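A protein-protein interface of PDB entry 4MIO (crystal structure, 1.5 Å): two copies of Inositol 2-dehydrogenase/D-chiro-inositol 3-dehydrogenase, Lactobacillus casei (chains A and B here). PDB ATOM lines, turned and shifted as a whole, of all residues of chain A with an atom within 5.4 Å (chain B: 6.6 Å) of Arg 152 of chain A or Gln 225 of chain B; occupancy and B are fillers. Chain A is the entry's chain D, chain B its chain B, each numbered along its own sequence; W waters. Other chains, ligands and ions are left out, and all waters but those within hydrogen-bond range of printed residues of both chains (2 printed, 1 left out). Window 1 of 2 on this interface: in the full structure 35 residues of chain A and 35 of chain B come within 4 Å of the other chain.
NH1 of Arg 152 of chain A lies within hydrogen-bond range of O of Ala 153 of chain B. NH1 of Arg 152 of chain B is in hydrogen-bond range of O of Ala 153 of chain A (3.0 Å). The backbone carbonyl oxygen (O) of Gln 225 of chain A is in hydrogen-bond range of the guanidinium group (NH2) of Arg 152 of chain B, at 3.0 Å. The side-chain hydroxyl (OG) of Ser 154 of chain B lies within hydrogen-bond range of the guanidinium group (NH1) of Arg 152 of chain A (3.4 Å). The backbone carbonyl oxygen (O) of Gln 225 of chain B is in hydrogen-bond range of the guanidinium group (NH2) of Arg 152 of chain A (3.0 Å).
The backbone carbonyl oxygen (O) of Ser 154 of chain A is in hydrogen-bond range of the backbone NH (N) of Lys 239 of chain A (3.0 Å). N of Glu 241 of chain A lies within hydrogen-bond range of O of Arg 152 of chain A (2.9 Å). N of Val 226 of chain B sits at hydrogen-bond distance from O of Ala 214 of chain B (2.8 Å). The backbone carbonyl oxygen (O) of Val 223 of chain B lies within hydrogen-bond range of the backbone NH (N) of Val 151 of chain B, at 2.9 Å. O of Gln 225 of chain A sits at hydrogen-bond distance from N of Ala 153 of chain A (3.0 Å). The guanidinium group of Arg 152 of chain A is in hydrogen-bond range of the side-chain amide oxygen of Gln 225 of chain A.
Among the printed residues, pairs that only touch across the chains: Leu 213 of chain A with Val 223 of chain B (3.6 Å), Arg 152 of chain A with Leu 227 of chain B (3.7 Å), Ile 243 of chain A with Leu 227 of chain B (3.7 Å), Ser 154 of chain A with Arg 152 of chain B (3.7 Å), Arg 152 of chain A with Val 226 of chain B (3.9 Å), Gln 225 of chain A with Gln 225 of chain B (3.9 Å), Leu 213 of chain A with Gln 225 of chain B (3.9 Å) and Gln 225 of chain A with Leu 213 of chain B (3.9 Å).
Arg 152 of chain A touches just these residues of chain B: Ala 153 (3.0 Å), Ser 154 (3.4 Å), Gln 225 (3.0 Å), Val 226 (3.9 Å) and Leu 227 (3.7 Å). Gln 225 of chain B touches three residues of chain A. Printed residues of chain A within 4 Å of Leu 213 of chain B: Gln 225. Printed residues of chain B within 4 Å of Leu 213 of chain A: Val 223 and Gln 225. Of the printed residues of chain A, Ala 153 of chain B touches Arg 152. Thr 215 of chain A touches none of the printed residues of chain B. Leu 240 of chain A touches none of the printed residues of chain B. The nearest residue of chain B that does not touch Arg 152 of chain A is Arg 152 of chain B (4.4 Å). The nearest printed residue of chain A that does not touch Ser 154 of chain B is Glu 241 of chain A (4.9 Å).
Hydrophobic or aromatic side chains of chain B within 4 Å of the printed part of chain A: Leu 213, Val 223 and Leu 227. Of the 13 printed residues of chain A, 6 touch a printed residue of chain B. Hydrophobic or aromatic side chains of chain A within 4 Å of the printed part of chain B: Leu 213 and Ile 243. Among the printed residues, no Asp or Glu carboxylate lies within 4 Å of a Lys or Arg side-chain nitrogen of the other chain.
Arg 152 of chain A touches Ala 153 of chain B, and with the chains exchanged Ala 153 of chain A touches Arg 152 of chain B. Arg 152 of chain A touches Ser 154 of chain B, and with the chains exchanged Ser 154 of chain A touches Arg 152 of chain B. Arg 152 of chain A touches Gln 225 of chain B, and with the chains exchanged Gln 225 of chain A touches Arg 152 of chain B. Gln 225 of chain B touches its own counterpart, Gln 225 of chain A. Positions printed for both chains: 150, 151, 152, 153, 154, 213, 215 and 225.
Water W2 lies within hydrogen-bond range of OE2 of Glu 241 of chain A and OG of Ser 154 of chain B. Water W1 lies within hydrogen-bond range of the side-chain amide nitrogen of Gln 225 of chain A, the backbone carbonyl oxygen of Ala 214 of chain B, the backbone NH of Val 226 of chain B and the side-chain hydroxyl of Thr 215 of chain B.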
ATOM      1  N   VAL A 150     -11.521  13.729  11.870  1.00  0.00           N
ATOM      2  CA  VAL A 150     -10.246  14.261  11.441  1.00  0.00           C
ATOM      3  C   VAL A 150     -10.352  15.792  11.355  1.00  0.00           C
ATOM      4  O   VAL A 150     -11.363  16.304  10.980  1.00  0.00           O
ATOM      5  CB  VAL A 150      -9.826  13.722  10.068  1.00  0.00           C
ATOM      6  CG1 VAL A 150      -8.568  14.350   9.587  1.00  0.00           C
ATOM      7  CG2 VAL A 150      -9.660  12.199  10.103  1.00  0.00           C
ATOM      8  N   VAL A 151      -9.291  16.470  11.745  1.00  0.00           N
ATOM      9  CA  VAL A 151      -9.170  17.904  11.581  1.00  0.00           C
ATOM     10  C   VAL A 151      -7.955  18.169  10.698  1.00  0.00           C
ATOM     11  O   VAL A 151      -6.940  17.610  10.889  1.00  0.00           O
ATOM     12  CB  VAL A 151      -9.008  18.636  12.913  1.00  0.00           C
ATOM     13  CG1 VAL A 151      -8.851  20.149  12.701  1.00  0.00           C
ATOM     14  CG2 VAL A 151     -10.165  18.383  13.802  1.00  0.00           C
ATOM     15  N   ARG A 152      -8.142  18.994   9.684  1.00  0.00           N
ATOM     16  CA  ARG A 152      -7.033  19.427   8.882  1.00  0.00           C
ATOM     17  C   ARG A 152      -6.868  20.931   9.009  1.00  0.00           C
ATOM     18  O   ARG A 152      -7.792  21.651   8.866  1.00  0.00           O
ATOM     19  CB  ARG A 152      -7.189  19.009   7.418  1.00  0.00           C
ATOM     20  CG  ARG A 152      -7.255  17.533   7.242  1.00  0.00           C
ATOM     21  CD  ARG A 152      -7.268  17.107   5.813  1.00  0.00           C
ATOM     22  NE  ARG A 152      -6.235  16.133   5.547  1.00  0.00           N
ATOM     23  CZ  ARG A 152      -6.027  15.602   4.367  1.00  0.00           C
ATOM     24  NH1 ARG A 152      -6.807  15.905   3.367  1.00  0.00           N
ATOM     25  NH2 ARG A 152      -5.087  14.701   4.230  1.00  0.00           N
ATOM     26  N   ALA A 153      -5.660  21.350   9.276  1.00  0.00           N
ATOM     27  CA  ALA A 153      -5.379  22.753   9.507  1.00  0.00           C
ATOM     28  C   ALA A 153      -4.078  23.191   8.844  1.00  0.00           C
ATOM     29  O   ALA A 153      -3.188  22.434   8.675  1.00  0.00           O
ATOM     30  CB  ALA A 153      -5.319  23.047  10.990  1.00  0.00           C
ATOM     31  N   SER A 154      -4.044  24.460   8.486  1.00  0.00           N
ATOM     32  CA  SER A 154      -2.840  25.079   7.989  1.00  0.00           C
ATOM     33  C   SER A 154      -2.534  26.368   8.766  1.00  0.00           C
ATOM     34  O   SER A 154      -3.407  27.122   9.061  1.00  0.00           O
ATOM     35  CB  SER A 154      -2.960  25.428   6.485  1.00  0.00           C
ATOM     36  OG  SER A 154      -3.149  24.304   5.693  1.00  0.00           O
ATOM     37  N   LEU A 213       5.103  19.141   9.339  1.00  0.00           N
ATOM     38  CA  LEU A 213       3.811  18.500   9.485  1.00  0.00           C
ATOM     39  C   LEU A 213       3.655  17.967  10.906  1.00  0.00           C
ATOM     40  O   LEU A 213       4.516  17.290  11.383  1.00  0.00           O
ATOM     41  CB  LEU A 213       3.631  17.360   8.480  1.00  0.00           C
ATOM     42  CG  LEU A 213       3.693  17.737   7.005  1.00  0.00           C
ATOM     43  CD1 LEU A 213       3.796  16.506   6.137  1.00  0.00           C
ATOM     44  CD2 LEU A 213       2.473  18.539   6.596  1.00  0.00           C
ATOM     45  N   THR A 215       1.093  15.821  13.397  1.00  0.00           N
ATOM     46  CA  THR A 215      -0.061  14.971  13.622  1.00  0.00           C
ATOM     47  C   THR A 215      -0.311  14.834  15.106  1.00  0.00           C
ATOM     48  O   THR A 215       0.532  14.401  15.810  1.00  0.00           O
ATOM     49  CB  THR A 215       0.146  13.570  13.032  1.00  0.00           C
ATOM     50  OG1 THR A 215       0.336  13.656  11.634  1.00  0.00           O
ATOM     51  CG2 THR A 215      -1.064  12.713  13.297  1.00  0.00           C
ATOM     52  N   GLN A 225      -4.213  16.872  11.583  1.00  0.00           N
ATOM     53  CA  GLN A 225      -3.083  17.078  10.694  1.00  0.00           C
ATOM     54  C   GLN A 225      -2.868  18.566  10.431  1.00  0.00           C
ATOM     55  O   GLN A 225      -3.644  19.162   9.754  1.00  0.00           O
ATOM     56  CB  GLN A 225      -3.329  16.380   9.347  1.00  0.00           C
ATOM     57  CG  GLN A 225      -3.415  14.864   9.425  1.00  0.00           C
ATOM     58  CD  GLN A 225      -3.576  14.209   8.061  1.00  0.00           C
ATOM     59  OE1 GLN A 225      -4.288  14.697   7.223  1.00  0.00           O
ATOM     60  NE2 GLN A 225      -2.906  13.114   7.867  1.00  0.00           N
ATOM     61  N   LYS A 239      -6.088  28.092   8.007  1.00  0.00           N
ATOM     62  CA  LYS A 239      -7.137  27.245   7.455  1.00  0.00           C
ATOM     63  C   LYS A 239      -7.539  26.166   8.484  1.00  0.00           C
ATOM     64  O   LYS A 239      -6.744  25.703   9.203  1.00  0.00           O
ATOM     65  CB  LYS A 239      -6.672  26.565   6.175  1.00  0.00           C
ATOM     66  CG  LYS A 239      -6.144  27.456   5.109  1.00  0.00           C
ATOM     67  CD  LYS A 239      -5.713  26.639   3.886  1.00  0.00           C
ATOM     68  CE  LYS A 239      -5.060  27.494   2.798  1.00  0.00           C
ATOM     69  NZ  LYS A 239      -4.830  26.745   1.606  1.00  0.00           N
ATOM     70  N   LEU A 240      -8.817  25.835   8.482  1.00  0.00           N
ATOM     71  CA  LEU A 240      -9.381  24.862   9.396  1.00  0.00           C
ATOM     72  C   LEU A 240     -10.528  24.118   8.720  1.00  0.00           C
ATOM     73  O   LEU A 240     -11.441  24.715   8.272  1.00  0.00           O
ATOM     74  CB  LEU A 240      -9.861  25.519  10.657  1.00  0.00           C
ATOM     75  CG  LEU A 240     -10.501  24.671  11.741  1.00  0.00           C
ATOM     76  CD1 LEU A 240      -9.524  23.681  12.305  1.00  0.00           C
ATOM     77  CD2 LEU A 240     -11.057  25.556  12.770  1.00  0.00           C
ATOM     78  N   GLU A 241     -10.420  22.808   8.707  1.00  0.00           N
ATOM     79  CA  GLU A 241     -11.427  21.940   8.174  1.00  0.00           C
ATOM     80  C   GLU A 241     -11.689  20.797   9.163  1.00  0.00           C
ATOM     81  O   GLU A 241     -10.806  20.163   9.592  1.00  0.00           O
ATOM     82  CB  GLU A 241     -10.987  21.405   6.829  1.00  0.00           C
ATOM     83  CG  GLU A 241     -11.810  20.278   6.263  1.00  0.00           C
ATOM     84  CD  GLU A 241     -11.203  19.695   4.987  1.00  0.00           C
ATOM     85  OE1 GLU A 241     -10.008  19.764   4.821  1.00  0.00           O
ATOM     86  OE2 GLU A 241     -11.928  19.163   4.140  1.00  0.00           O
ATOM     87  N   VAL A 242     -12.948  20.617   9.530  1.00  0.00           N
ATOM     88  CA  VAL A 242     -13.323  19.541  10.409  1.00  0.00           C
ATOM     89  C   VAL A 242     -14.130  18.502   9.611  1.00  0.00           C
ATOM     90  O   VAL A 242     -15.118  18.829   9.044  1.00  0.00           O
ATOM     91  CB  VAL A 242     -14.128  20.012  11.638  1.00  0.00           C
ATOM     92  CG1 VAL A 242     -14.499  18.840  12.527  1.00  0.00           C
ATOM     93  CG2 VAL A 242     -13.358  21.049  12.414  1.00  0.00           C
ATOM     94  N   ILE A 243     -13.617  17.295   9.606  1.00  0.00           N
ATOM     95  CA  ILE A 243     -14.257  16.181   8.920  1.00  0.00           C
ATOM     96  C   ILE A 243     -15.101  15.371   9.919  1.00  0.00           C
ATOM     97  O   ILE A 243     -14.585  14.794  10.811  1.00  0.00           O
ATOM     98  CB  ILE A 243     -13.193  15.291   8.224  1.00  0.00           C
ATOM     99  CG1 ILE A 243     -12.462  16.073   7.110  1.00  0.00           C
ATOM    100  CG2 ILE A 243     -13.848  14.084   7.632  1.00  0.00           C
ATOM    101  CD1 ILE A 243     -11.206  16.683   7.507  1.00  0.00           C
ATOM    102  N   VAL B 150       4.462  19.500  -0.197  1.00  0.00           N
ATOM    103  CA  VAL B 150       3.411  18.734   0.421  1.00  0.00           C
ATOM    104  C   VAL B 150       2.202  18.714  -0.517  1.00  0.00           C
ATOM    105  O   VAL B 150       1.910  19.651  -1.179  1.00  0.00           O
ATOM    106  CB  VAL B 150       3.001  19.318   1.794  1.00  0.00           C
ATOM    107  CG1 VAL B 150       1.930  18.495   2.436  1.00  0.00           C
ATOM    108  CG2 VAL B 150       4.157  19.363   2.735  1.00  0.00           C
ATOM    109  N   VAL B 151       1.537  17.571  -0.568  1.00  0.00           N
ATOM    110  CA  VAL B 151       0.266  17.455  -1.227  1.00  0.00           C
ATOM    111  C   VAL B 151      -0.790  16.994  -0.203  1.00  0.00           C
ATOM    112  O   VAL B 151      -0.550  16.076   0.521  1.00  0.00           O
ATOM    113  CB  VAL B 151       0.312  16.432  -2.391  1.00  0.00           C
ATOM    114  CG1 VAL B 151      -1.043  16.291  -3.054  1.00  0.00           C
ATOM    115  CG2 VAL B 151       1.334  16.841  -3.424  1.00  0.00           C
ATOM    116  N   ARG B 152      -1.920  17.677  -0.178  1.00  0.00           N
ATOM    117  CA  ARG B 152      -3.003  17.310   0.695  1.00  0.00           C
ATOM    118  C   ARG B 152      -4.204  17.027  -0.186  1.00  0.00           C
ATOM    119  O   ARG B 152      -4.580  17.832  -0.963  1.00  0.00           O
ATOM    120  CB  ARG B 152      -3.332  18.422   1.666  1.00  0.00           C
ATOM    121  CG  ARG B 152      -2.218  18.808   2.566  1.00  0.00           C
ATOM    122  CD  ARG B 152      -2.709  19.649   3.731  1.00  0.00           C
ATOM    123  NE  ARG B 152      -2.306  19.068   4.958  1.00  0.00           N
ATOM    124  CZ  ARG B 152      -2.577  19.532   6.157  1.00  0.00           C
ATOM    125  NH1 ARG B 152      -3.287  20.609   6.302  1.00  0.00           N
ATOM    126  NH2 ARG B 152      -2.092  18.913   7.186  1.00  0.00           N
ATOM    127  N   ALA B 153      -4.783  15.846  -0.040  1.00  0.00           N
ATOM    128  CA  ALA B 153      -5.844  15.411  -0.922  1.00  0.00           C
ATOM    129  C   ALA B 153      -6.932  14.697  -0.146  1.00  0.00           C
ATOM    130  O   ALA B 153      -6.691  14.229   0.916  1.00  0.00           O
ATOM    131  CB  ALA B 153      -5.293  14.502  -1.987  1.00  0.00           C
ATOM    132  N   SER B 154      -8.119  14.676  -0.727  1.00  0.00           N
ATOM    133  CA  SER B 154      -9.242  13.960  -0.164  1.00  0.00           C
ATOM    134  C   SER B 154      -9.955  13.156  -1.245  1.00  0.00           C
ATOM    135  O   SER B 154     -10.164  13.631  -2.296  1.00  0.00           O
ATOM    136  CB  SER B 154     -10.270  14.899   0.490  1.00  0.00           C
ATOM    137  OG  SER B 154      -9.731  15.617   1.565  1.00  0.00           O
ATOM    138  N   MET B 181      -0.583  10.643  -8.043  1.00  0.00           N
ATOM    139  CA  MET B 181       0.382  11.498  -7.395  1.00  0.00           C
ATOM    140  C   MET B 181       1.798  11.414  -7.996  1.00  0.00           C
ATOM    141  O   MET B 181       2.451  12.390  -8.121  1.00  0.00           O
ATOM    142  CB  MET B 181       0.397  11.290  -5.892  1.00  0.00           C
ATOM    143  CG  MET B 181      -0.904  11.524  -5.228  1.00  0.00           C
ATOM    144  SD  MET B 181      -1.487  13.192  -5.435  1.00  0.00           S
ATOM    145  CE  MET B 181      -3.053  13.059  -4.592  1.00  0.00           C
ATOM    146  N   LEU B 213      -6.315   7.466   6.782  1.00  0.00           N
ATOM    147  CA  LEU B 213      -5.346   8.447   6.365  1.00  0.00           C
ATOM    148  C   LEU B 213      -4.158   7.763   5.732  1.00  0.00           C
ATOM    149  O   LEU B 213      -3.560   6.947   6.312  1.00  0.00           O
ATOM    150  CB  LEU B 213      -4.870   9.266   7.561  1.00  0.00           C
ATOM    151  CG  LEU B 213      -5.941  10.115   8.215  1.00  0.00           C
ATOM    152  CD1 LEU B 213      -5.452  10.665   9.535  1.00  0.00           C
ATOM    153  CD2 LEU B 213      -6.347  11.223   7.314  1.00  0.00           C
ATOM    154  N   ALA B 214      -3.855   8.142   4.511  1.00  0.00           N
ATOM    155  CA  ALA B 214      -2.724   7.595   3.811  1.00  0.00           C
ATOM    156  C   ALA B 214      -1.621   8.637   3.673  1.00  0.00           C
ATOM    157  O   ALA B 214      -1.878   9.704   3.213  1.00  0.00           O
ATOM    158  CB  ALA B 214      -3.135   7.120   2.469  1.00  0.00           C
ATOM    159  N   THR B 215      -0.446   8.277   4.089  1.00  0.00           N
ATOM    160  CA  THR B 215       0.697   9.137   3.935  1.00  0.00           C
ATOM    161  C   THR B 215       1.735   8.490   3.042  1.00  0.00           C
ATOM    162  O   THR B 215       2.162   7.412   3.301  1.00  0.00           O
ATOM    163  CB  THR B 215       1.310   9.485   5.295  1.00  0.00           C
ATOM    164  OG1 THR B 215       0.316  10.114   6.102  1.00  0.00           O
ATOM    165  CG2 THR B 215       2.489  10.409   5.086  1.00  0.00           C
ATOM    166  N   LEU B 216       2.075   9.157   1.960  1.00  0.00           N
ATOM    167  CA  LEU B 216       3.091   8.679   1.050  1.00  0.00           C
ATOM    168  C   LEU B 216       4.277   9.638   1.007  1.00  0.00           C
ATOM    169  O   LEU B 216       4.107  10.805   1.060  1.00  0.00           O
ATOM    170  CB  LEU B 216       2.538   8.506  -0.364  1.00  0.00           C
ATOM    171  CG  LEU B 216       1.423   7.488  -0.622  1.00  0.00           C
ATOM    172  CD1 LEU B 216       0.088   8.025  -0.198  1.00  0.00           C
ATOM    173  CD2 LEU B 216       1.419   7.092  -2.057  1.00  0.00           C
ATOM    174  N   VAL B 223       5.788  15.028   0.749  1.00  0.00           N
ATOM    175  CA  VAL B 223       4.885  14.218   1.530  1.00  0.00           C
ATOM    176  C   VAL B 223       3.432  14.416   1.056  1.00  0.00           C
ATOM    177  O   VAL B 223       2.987  15.514   0.881  1.00  0.00           O
ATOM    178  CB  VAL B 223       4.994  14.504   3.036  1.00  0.00           C
ATOM    179  CG1 VAL B 223       3.918  13.751   3.817  1.00  0.00           C
ATOM    180  CG2 VAL B 223       6.381  14.176   3.562  1.00  0.00           C
ATOM    181  N   ILE B 224       2.757  13.309   0.803  1.00  0.00           N
ATOM    182  CA  ILE B 224       1.404  13.312   0.350  1.00  0.00           C
ATOM    183  C   ILE B 224       0.500  12.789   1.456  1.00  0.00           C
ATOM    184  O   ILE B 224       0.711  11.720   1.925  1.00  0.00           O
ATOM    185  CB  ILE B 224       1.221  12.400  -0.892  1.00  0.00           C
ATOM    186  CG1 ILE B 224       2.124  12.849  -2.035  1.00  0.00           C
ATOM    187  CG2 ILE B 224      -0.194  12.361  -1.346  1.00  0.00           C
ATOM    188  CD1 ILE B 224       2.690  11.742  -2.856  1.00  0.00           C
ATOM    189  N   GLN B 225      -0.486  13.579   1.824  1.00  0.00           N
ATOM    190  CA  GLN B 225      -1.464  13.197   2.825  1.00  0.00           C
ATOM    191  C   GLN B 225      -2.846  13.083   2.196  1.00  0.00           C
ATOM    192  O   GLN B 225      -3.400  14.045   1.811  1.00  0.00           O
ATOM    193  CB  GLN B 225      -1.503  14.224   3.957  1.00  0.00           C
ATOM    194  CG  GLN B 225      -0.215  14.411   4.724  1.00  0.00           C
ATOM    195  CD  GLN B 225      -0.325  15.483   5.815  1.00  0.00           C
ATOM    196  OE1 GLN B 225      -0.912  16.509   5.615  1.00  0.00           O
ATOM    197  NE2 GLN B 225       0.231  15.206   6.951  1.00  0.00           N
ATOM    198  N   VAL B 226      -3.358  11.863   2.097  1.00  0.00           N
ATOM    199  CA  VAL B 226      -4.692  11.649   1.566  1.00  0.00           C
ATOM    200  C   VAL B 226      -5.674  11.212   2.649  1.00  0.00           C
ATOM    201  O   VAL B 226      -5.373  10.338   3.404  1.00  0.00           O
ATOM    202  CB  VAL B 226      -4.733  10.571   0.470  1.00  0.00           C
ATOM    203  CG1 VAL B 226      -6.077  10.540  -0.185  1.00  0.00           C
ATOM    204  CG2 VAL B 226      -3.630  10.790  -0.548  1.00  0.00           C
ATOM    205  N   LEU B 227      -6.812  11.875   2.688  1.00  0.00           N
ATOM    206  CA  LEU B 227      -7.928  11.473   3.510  1.00  0.00           C
ATOM    207  C   LEU B 227      -8.866  10.630   2.641  1.00  0.00           C
ATOM    208  O   LEU B 227      -9.323  11.081   1.649  1.00  0.00           O
ATOM    209  CB  LEU B 227      -8.689  12.687   4.031  1.00  0.00           C
ATOM    210  CG  LEU B 227     -10.059  12.411   4.644  1.00  0.00           C
ATOM    211  CD1 LEU B 227      -9.925  11.642   5.897  1.00  0.00           C
ATOM    212  CD2 LEU B 227     -10.790  13.699   4.890  1.00  0.00           C
HETATM  213  O   HOH W   1      -2.846  11.450   5.437  1.00  0.00           O
HETATM  214  O   HOH W   2     -12.000  16.640   2.940  1.00  0.00           O
